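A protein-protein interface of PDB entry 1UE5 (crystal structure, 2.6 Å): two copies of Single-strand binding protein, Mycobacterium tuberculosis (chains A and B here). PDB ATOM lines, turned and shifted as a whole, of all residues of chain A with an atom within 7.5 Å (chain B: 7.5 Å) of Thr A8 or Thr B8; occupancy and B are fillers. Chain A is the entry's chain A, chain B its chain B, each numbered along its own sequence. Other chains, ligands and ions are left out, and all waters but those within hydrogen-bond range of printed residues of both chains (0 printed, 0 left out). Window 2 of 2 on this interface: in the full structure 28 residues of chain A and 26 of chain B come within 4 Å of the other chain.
Hydrophobic or aromatic side chains of chain B within 4 Å of the printed part of chain A: Ile B78. Along chain B the printed residues that touch a printed residue of chain A span positions 8 to 105. Of the 15 printed residues of chain A, 4 touch a printed residue of chain B. Hydrophobic or aromatic side chains of chain A that line the printed part of chain B: Val A10 and Ile A78. Among the printed residues, 5 pairs touch across the chains.
Thr B8 touches its own counterpart, Thr A8. Ile A78 touches its own counterpart, Ile B78. Ser A80 touches Ile B78, but with the chains exchanged Ile A78 does not touch Ser B80 (4.6 Å). 13 positions are printed for both chains.
The side-chain hydroxyl (OG1) of Thr A8 lies within hydrogen-bond range of the side-chain hydroxyl (OG1) of Thr B8 (3.0 Å).
Among the printed residues, pairs that only touch across the chains: Val A10 with Glu B105, Ile A78 with Glu B105, Ile A78 with Ile B78 and Ser A80 with Ile B78.
O of Val A10 sits at hydrogen-bond distance from OG of Ser A35. N of Ser B80 is in hydrogen-bond range of O of Glu B105, 2.9 Å away.
Thr A8 touches one residue of chain B. Of the printed residues of chain B, Ile A78 touches Ile B78 and Glu B105. Of the printed residues of chain B, Ser A80 touches Ile B78 (3.97 Å). Of chain A, only Thr A8 (3.0 Å) comes within 4 Å of Thr B8. Leu B55 touches none of the printed residues of chain A. Val B101 touches none of the printed residues of chain A. Printed residues of chain A within 4 Å of Glu B105: Val A10 (3.2 Å) and Ile A78 (3.4 Å). The nearest residue of chain B that does not touch Thr A8 is Ser B80 (4.3 Å). The nearest printed residue of chain A that does not touch Ile B78 is Val A79 (4.4 Å).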
ATOM      1  N   THR A   6      15.013 -14.760 -21.399  1.00  0.00           N
ATOM      2  CA  THR A   6      15.338 -13.466 -20.809  1.00  0.00           C
ATOM      3  C   THR A   6      15.666 -12.469 -21.919  1.00  0.00           C
ATOM      4  O   THR A   6      15.955 -12.856 -23.053  1.00  0.00           O
ATOM      5  CB  THR A   6      16.562 -13.578 -19.861  1.00  0.00           C
ATOM      6  OG1 THR A   6      17.661 -14.176 -20.564  1.00  0.00           O
ATOM      7  CG2 THR A   6      16.218 -14.427 -18.646  1.00  0.00           C
ATOM      8  N   ILE A   7      15.599 -11.182 -21.604  1.00  0.00           N
ATOM      9  CA  ILE A   7      15.930 -10.174 -22.587  1.00  0.00           C
ATOM     10  C   ILE A   7      16.595  -8.984 -21.941  1.00  0.00           C
ATOM     11  O   ILE A   7      16.523  -8.786 -20.725  1.00  0.00           O
ATOM     12  CB  ILE A   7      14.693  -9.656 -23.336  1.00  0.00           C
ATOM     13  CG1 ILE A   7      13.747  -8.968 -22.359  1.00  0.00           C
ATOM     14  CG2 ILE A   7      14.007 -10.801 -24.072  1.00  0.00           C
ATOM     15  CD1 ILE A   7      12.644  -8.204 -23.052  1.00  0.00           C
ATOM     16  N   THR A   8      17.251  -8.190 -22.771  1.00  0.00           N
ATOM     17  CA  THR A   8      17.920  -6.998 -22.304  1.00  0.00           C
ATOM     18  C   THR A   8      17.390  -5.922 -23.204  1.00  0.00           C
ATOM     19  O   THR A   8      17.432  -6.065 -24.420  1.00  0.00           O
ATOM     20  CB  THR A   8      19.444  -7.099 -22.469  1.00  0.00           C
ATOM     21  OG1 THR A   8      19.960  -8.095 -21.575  1.00  0.00           O
ATOM     22  CG2 THR A   8      20.094  -5.764 -22.162  1.00  0.00           C
ATOM     23  N   ILE A   9      16.868  -4.858 -22.609  1.00  0.00           N
ATOM     24  CA  ILE A   9      16.322  -3.757 -23.391  1.00  0.00           C
ATOM     25  C   ILE A   9      16.872  -2.447 -22.884  1.00  0.00           C
ATOM     26  O   ILE A   9      17.091  -2.284 -21.680  1.00  0.00           O
ATOM     27  CB  ILE A   9      14.770  -3.695 -23.314  1.00  0.00           C
ATOM     28  CG1 ILE A   9      14.250  -2.500 -24.126  1.00  0.00           C
ATOM     29  CG2 ILE A   9      14.325  -3.564 -21.869  1.00  0.00           C
ATOM     30  CD1 ILE A   9      12.724  -2.400 -24.216  1.00  0.00           C
ATOM     31  N   VAL A  10      17.106  -1.528 -23.815  1.00  0.00           N
ATOM     32  CA  VAL A  10      17.609  -0.197 -23.498  1.00  0.00           C
ATOM     33  C   VAL A  10      16.576   0.788 -24.012  1.00  0.00           C
ATOM     34  O   VAL A  10      16.123   0.678 -25.146  1.00  0.00           O
ATOM     35  CB  VAL A  10      18.940   0.083 -24.199  1.00  0.00           C
ATOM     36  CG1 VAL A  10      19.451   1.459 -23.808  1.00  0.00           C
ATOM     37  CG2 VAL A  10      19.946  -0.988 -23.839  1.00  0.00           C
ATOM     38  N   SER A  35      11.638   1.636 -25.955  1.00  0.00           N
ATOM     39  CA  SER A  35      12.901   1.392 -26.638  1.00  0.00           C
ATOM     40  C   SER A  35      12.835   1.887 -28.079  1.00  0.00           C
ATOM     41  O   SER A  35      12.378   1.159 -28.954  1.00  0.00           O
ATOM     42  CB  SER A  35      13.209  -0.109 -26.620  1.00  0.00           C
ATOM     43  OG  SER A  35      14.307  -0.427 -27.460  1.00  0.00           O
ATOM     44  N   LEU A  53       9.338  -0.046 -29.121  1.00  0.00           N
ATOM     45  CA  LEU A  53       8.832  -1.182 -28.370  1.00  0.00           C
ATOM     46  C   LEU A  53       8.657  -0.777 -26.914  1.00  0.00           C
ATOM     47  O   LEU A  53       9.625  -0.440 -26.237  1.00  0.00           O
ATOM     48  CB  LEU A  53       9.846  -2.316 -28.501  1.00  0.00           C
ATOM     49  CG  LEU A  53       9.685  -3.639 -27.772  1.00  0.00           C
ATOM     50  CD1 LEU A  53       8.730  -4.540 -28.529  1.00  0.00           C
ATOM     51  CD2 LEU A  53      11.054  -4.292 -27.669  1.00  0.00           C
ATOM     52  N   LEU A  55       7.758  -1.876 -23.235  1.00  0.00           N
ATOM     53  CA  LEU A  55       7.637  -3.038 -22.347  1.00  0.00           C
ATOM     54  C   LEU A  55       7.381  -2.739 -20.876  1.00  0.00           C
ATOM     55  O   LEU A  55       8.173  -2.075 -20.200  1.00  0.00           O
ATOM     56  CB  LEU A  55       8.885  -3.922 -22.443  1.00  0.00           C
ATOM     57  CG  LEU A  55       9.138  -4.624 -23.774  1.00  0.00           C
ATOM     58  CD1 LEU A  55      10.422  -5.395 -23.704  1.00  0.00           C
ATOM     59  CD2 LEU A  55       7.988  -5.544 -24.084  1.00  0.00           C
ATOM     60  N   VAL A  77      17.663   3.807 -19.701  1.00  0.00           N
ATOM     61  CA  VAL A  77      18.126   2.715 -18.853  1.00  0.00           C
ATOM     62  C   VAL A  77      18.424   1.398 -19.554  1.00  0.00           C
ATOM     63  O   VAL A  77      17.895   1.116 -20.628  1.00  0.00           O
ATOM     64  CB  VAL A  77      17.089   2.410 -17.780  1.00  0.00           C
ATOM     65  CG1 VAL A  77      16.789   3.654 -16.969  1.00  0.00           C
ATOM     66  CG2 VAL A  77      15.827   1.890 -18.439  1.00  0.00           C
ATOM     67  N   ILE A  78      19.268   0.592 -18.916  1.00  0.00           N
ATOM     68  CA  ILE A  78      19.625  -0.730 -19.418  1.00  0.00           C
ATOM     69  C   ILE A  78      18.899  -1.729 -18.513  1.00  0.00           C
ATOM     70  O   ILE A  78      19.186  -1.818 -17.317  1.00  0.00           O
ATOM     71  CB  ILE A  78      21.130  -0.980 -19.319  1.00  0.00           C
ATOM     72  CG1 ILE A  78      21.881   0.190 -19.947  1.00  0.00           C
ATOM     73  CG2 ILE A  78      21.485  -2.282 -20.026  1.00  0.00           C
ATOM     74  CD1 ILE A  78      23.369   0.065 -19.861  1.00  0.00           C
ATOM     75  N   VAL A  79      17.955  -2.467 -19.091  1.00  0.00           N
ATOM     76  CA  VAL A  79      17.163  -3.429 -18.344  1.00  0.00           C
ATOM     77  C   VAL A  79      17.388  -4.885 -18.742  1.00  0.00           C
ATOM     78  O   VAL A  79      17.445  -5.231 -19.926  1.00  0.00           O
ATOM     79  CB  VAL A  79      15.660  -3.098 -18.478  1.00  0.00           C
ATOM     80  CG1 VAL A  79      14.806  -4.214 -17.872  1.00  0.00           C
ATOM     81  CG2 VAL A  79      15.371  -1.779 -17.791  1.00  0.00           C
ATOM     82  N   SER A  80      17.517  -5.728 -17.724  1.00  0.00           N
ATOM     83  CA  SER A  80      17.713  -7.159 -17.899  1.00  0.00           C
ATOM     84  C   SER A  80      16.687  -7.868 -17.035  1.00  0.00           C
ATOM     85  O   SER A  80      16.399  -7.436 -15.918  1.00  0.00           O
ATOM     86  CB  SER A  80      19.110  -7.582 -17.453  1.00  0.00           C
ATOM     87  OG  SER A  80      19.197  -9.000 -17.404  1.00  0.00           O
ATOM     88  N   GLY A  81      16.139  -8.959 -17.555  1.00  0.00           N
ATOM     89  CA  GLY A  81      15.141  -9.702 -16.819  1.00  0.00           C
ATOM     90  C   GLY A  81      14.545 -10.785 -17.684  1.00  0.00           C
ATOM     91  O   GLY A  81      15.067 -11.086 -18.755  1.00  0.00           O
ATOM     92  N   ARG A  82      13.448 -11.371 -17.226  1.00  0.00           N
ATOM     93  CA  ARG A  82      12.797 -12.427 -17.977  1.00  0.00           C
ATOM     94  C   ARG A  82      11.421 -12.000 -18.459  1.00  0.00           C
ATOM     95  O   ARG A  82      10.729 -11.255 -17.775  1.00  0.00           O
ATOM     96  CB  ARG A  82      12.695 -13.680 -17.108  1.00  0.00           C
ATOM     97  CG  ARG A  82      12.123 -13.424 -15.731  1.00  0.00           C
ATOM     98  CD  ARG A  82      12.233 -14.658 -14.852  1.00  0.00           C
ATOM     99  NE  ARG A  82      11.722 -14.408 -13.509  1.00  0.00           N
ATOM    100  CZ  ARG A  82      12.187 -13.467 -12.694  1.00  0.00           C
ATOM    101  NH1 ARG A  82      11.658 -13.314 -11.487  1.00  0.00           N
ATOM    102  NH2 ARG A  82      13.180 -12.677 -13.079  1.00  0.00           N
ATOM    103  N   VAL A 101       8.059  -7.814 -18.306  1.00  0.00           N
ATOM    104  CA  VAL A 101       9.429  -8.182 -17.993  1.00  0.00           C
ATOM    105  C   VAL A 101       9.606  -8.110 -16.497  1.00  0.00           C
ATOM    106  O   VAL A 101       9.286  -7.088 -15.883  1.00  0.00           O
ATOM    107  CB  VAL A 101      10.462  -7.209 -18.634  1.00  0.00           C
ATOM    108  CG1 VAL A 101      11.864  -7.600 -18.208  1.00  0.00           C
ATOM    109  CG2 VAL A 101      10.360  -7.237 -20.149  1.00  0.00           C
ATOM    110  N   THR B   6      26.513 -10.345 -29.362  1.00  0.00           N
ATOM    111  CA  THR B   6      26.247  -9.452 -28.242  1.00  0.00           C
ATOM    112  C   THR B   6      26.000 -10.153 -26.923  1.00  0.00           C
ATOM    113  O   THR B   6      25.402 -11.221 -26.890  1.00  0.00           O
ATOM    114  CB  THR B   6      25.016  -8.598 -28.529  1.00  0.00           C
ATOM    115  OG1 THR B   6      23.913  -9.464 -28.825  1.00  0.00           O
ATOM    116  CG2 THR B   6      25.264  -7.686 -29.713  1.00  0.00           C
ATOM    117  N   ILE B   7      26.448  -9.542 -25.831  1.00  0.00           N
ATOM    118  CA  ILE B   7      26.219 -10.123 -24.523  1.00  0.00           C
ATOM    119  C   ILE B   7      25.912  -9.070 -23.477  1.00  0.00           C
ATOM    120  O   ILE B   7      26.291  -7.907 -23.602  1.00  0.00           O
ATOM    121  CB  ILE B   7      27.428 -10.930 -24.005  1.00  0.00           C
ATOM    122  CG1 ILE B   7      28.371 -10.018 -23.226  1.00  0.00           C
ATOM    123  CG2 ILE B   7      28.169 -11.562 -25.157  1.00  0.00           C
ATOM    124  CD1 ILE B   7      29.317 -10.770 -22.352  1.00  0.00           C
ATOM    125  N   THR B   8      25.230  -9.500 -22.426  1.00  0.00           N
ATOM    126  CA  THR B   8      24.895  -8.617 -21.333  1.00  0.00           C
ATOM    127  C   THR B   8      25.531  -9.228 -20.084  1.00  0.00           C
ATOM    128  O   THR B   8      25.369 -10.417 -19.818  1.00  0.00           O
ATOM    129  CB  THR B   8      23.375  -8.494 -21.193  1.00  0.00           C
ATOM    130  OG1 THR B   8      22.836  -7.960 -22.413  1.00  0.00           O
ATOM    131  CG2 THR B   8      23.018  -7.564 -20.041  1.00  0.00           C
ATOM    132  N   ILE B   9      26.278  -8.418 -19.341  1.00  0.00           N
ATOM    133  CA  ILE B   9      26.965  -8.893 -18.147  1.00  0.00           C
ATOM    134  C   ILE B   9      26.775  -7.990 -16.934  1.00  0.00           C
ATOM    135  O   ILE B   9      26.801  -6.764 -17.043  1.00  0.00           O
ATOM    136  CB  ILE B   9      28.483  -9.048 -18.415  1.00  0.00           C
ATOM    137  CG1 ILE B   9      29.201  -9.493 -17.140  1.00  0.00           C
ATOM    138  CG2 ILE B   9      29.055  -7.734 -18.922  1.00  0.00           C
ATOM    139  CD1 ILE B   9      30.650  -9.878 -17.348  1.00  0.00           C
ATOM    140  N   VAL B  10      26.574  -8.616 -15.779  1.00  0.00           N
ATOM    141  CA  VAL B  10      26.393  -7.895 -14.528  1.00  0.00           C
ATOM    142  C   VAL B  10      27.582  -8.241 -13.635  1.00  0.00           C
ATOM    143  O   VAL B  10      28.045  -9.377 -13.624  1.00  0.00           O
ATOM    144  CB  VAL B  10      25.059  -8.294 -13.855  1.00  0.00           C
ATOM    145  CG1 VAL B  10      24.967  -7.700 -12.469  1.00  0.00           C
ATOM    146  CG2 VAL B  10      23.901  -7.798 -14.697  1.00  0.00           C
ATOM    147  N   SER B  35      32.082 -10.877 -12.872  1.00  0.00           N
ATOM    148  CA  SER B  35      30.738 -11.401 -12.696  1.00  0.00           C
ATOM    149  C   SER B  35      30.821 -12.643 -11.806  1.00  0.00           C
ATOM    150  O   SER B  35      31.543 -13.586 -12.125  1.00  0.00           O
ATOM    151  CB  SER B  35      30.149 -11.762 -14.067  1.00  0.00           C
ATOM    152  OG  SER B  35      28.811 -12.214 -13.957  1.00  0.00           O
ATOM    153  N   LEU B  55      35.781 -10.267 -17.412  1.00  0.00           N
ATOM    154  CA  LEU B  55      35.811  -9.814 -18.801  1.00  0.00           C
ATOM    155  C   LEU B  55      36.261  -8.356 -18.821  1.00  0.00           C
ATOM    156  O   LEU B  55      35.734  -7.528 -18.073  1.00  0.00           O
ATOM    157  CB  LEU B  55      34.422  -9.920 -19.440  1.00  0.00           C
ATOM    158  CG  LEU B  55      33.912 -11.279 -19.911  1.00  0.00           C
ATOM    159  CD1 LEU B  55      32.415 -11.209 -20.101  1.00  0.00           C
ATOM    160  CD2 LEU B  55      34.590 -11.670 -21.213  1.00  0.00           C
ATOM    161  N   ILE B  78      25.831  -3.069 -15.059  1.00  0.00           N
ATOM    162  CA  ILE B  78      25.215  -3.972 -16.021  1.00  0.00           C
ATOM    163  C   ILE B  78      25.709  -3.488 -17.390  1.00  0.00           C
ATOM    164  O   ILE B  78      25.543  -2.327 -17.758  1.00  0.00           O
ATOM    165  CB  ILE B  78      23.662  -3.947 -15.917  1.00  0.00           C
ATOM    166  CG1 ILE B  78      23.039  -4.432 -17.228  1.00  0.00           C
ATOM    167  CG2 ILE B  78      23.192  -2.578 -15.489  1.00  0.00           C
ATOM    168  CD1 ILE B  78      21.530  -4.441 -17.214  1.00  0.00           C
ATOM    169  N   VAL B  79      26.332  -4.388 -18.133  1.00  0.00           N
ATOM    170  CA  VAL B  79      26.919  -4.047 -19.419  1.00  0.00           C
ATOM    171  C   VAL B  79      26.336  -4.790 -20.614  1.00  0.00           C
ATOM    172  O   VAL B  79      26.117  -6.000 -20.564  1.00  0.00           O
ATOM    173  CB  VAL B  79      28.451  -4.322 -19.375  1.00  0.00           C
ATOM    174  CG1 VAL B  79      29.101  -4.026 -20.714  1.00  0.00           C
ATOM    175  CG2 VAL B  79      29.087  -3.497 -18.279  1.00  0.00           C
ATOM    176  N   SER B  80      26.084  -4.056 -21.691  1.00  0.00           N
ATOM    177  CA  SER B  80      25.583  -4.660 -22.916  1.00  0.00           C
ATOM    178  C   SER B  80      26.632  -4.313 -23.959  1.00  0.00           C
ATOM    179  O   SER B  80      27.007  -3.146 -24.105  1.00  0.00           O
ATOM    180  CB  SER B  80      24.226  -4.070 -23.311  1.00  0.00           C
ATOM    181  OG  SER B  80      23.650  -4.801 -24.383  1.00  0.00           O
ATOM    182  N   GLY B  81      27.122  -5.325 -24.664  1.00  0.00           N
ATOM    183  CA  GLY B  81      28.143  -5.079 -25.661  1.00  0.00           C
ATOM    184  C   GLY B  81      28.318  -6.177 -26.690  1.00  0.00           C
ATOM    185  O   GLY B  81      27.405  -6.973 -26.929  1.00  0.00           O
ATOM    186  N   ARG B  82      29.500  -6.209 -27.303  1.00  0.00           N
ATOM    187  CA  ARG B  82      29.818  -7.196 -28.326  1.00  0.00           C
ATOM    188  C   ARG B  82      31.194  -7.808 -28.109  1.00  0.00           C
ATOM    189  O   ARG B  82      32.179  -7.095 -27.920  1.00  0.00           O
ATOM    190  CB  ARG B  82      29.752  -6.551 -29.713  1.00  0.00           C
ATOM    191  CG  ARG B  82      28.336  -6.290 -30.211  1.00  0.00           C
ATOM    192  CD  ARG B  82      28.298  -5.161 -31.235  1.00  0.00           C
ATOM    193  NE  ARG B  82      28.779  -3.910 -30.648  1.00  0.00           N
ATOM    194  CZ  ARG B  82      30.004  -3.418 -30.808  1.00  0.00           C
ATOM    195  NH1 ARG B  82      30.890  -4.063 -31.552  1.00  0.00           N
ATOM    196  NH2 ARG B  82      30.347  -2.285 -30.212  1.00  0.00           N
ATOM    197  N   VAL B 101      35.198  -7.236 -24.436  1.00  0.00           N
ATOM    198  CA  VAL B 101      33.874  -6.720 -24.747  1.00  0.00           C
ATOM    199  C   VAL B 101      33.856  -5.246 -25.133  1.00  0.00           C
ATOM    200  O   VAL B 101      34.229  -4.386 -24.337  1.00  0.00           O
ATOM    201  CB  VAL B 101      32.924  -6.892 -23.545  1.00  0.00           C
ATOM    202  CG1 VAL B 101      31.582  -6.220 -23.828  1.00  0.00           C
ATOM    203  CG2 VAL B 101      32.740  -8.361 -23.252  1.00  0.00           C
ATOM    204  N   GLU B 105      26.418  -0.115 -24.210  1.00  0.00           N
ATOM    205  CA  GLU B 105      25.715   0.597 -23.155  1.00  0.00           C
ATOM    206  C   GLU B 105      26.160   0.044 -21.803  1.00  0.00           C
ATOM    207  O   GLU B 105      26.468  -1.146 -21.669  1.00  0.00           O
ATOM    208  CB  GLU B 105      24.206   0.406 -23.303  1.00  0.00           C
ATOM    209  CG  GLU B 105      23.632   0.916 -24.604  1.00  0.00           C
ATOM    210  CD  GLU B 105      22.897   2.217 -24.435  1.00  0.00           C
ATOM    211  OE1 GLU B 105      23.149   2.917 -23.433  1.00  0.00           O
ATOM    212  OE2 GLU B 105      22.072   2.542 -25.312  1.00  0.00           O
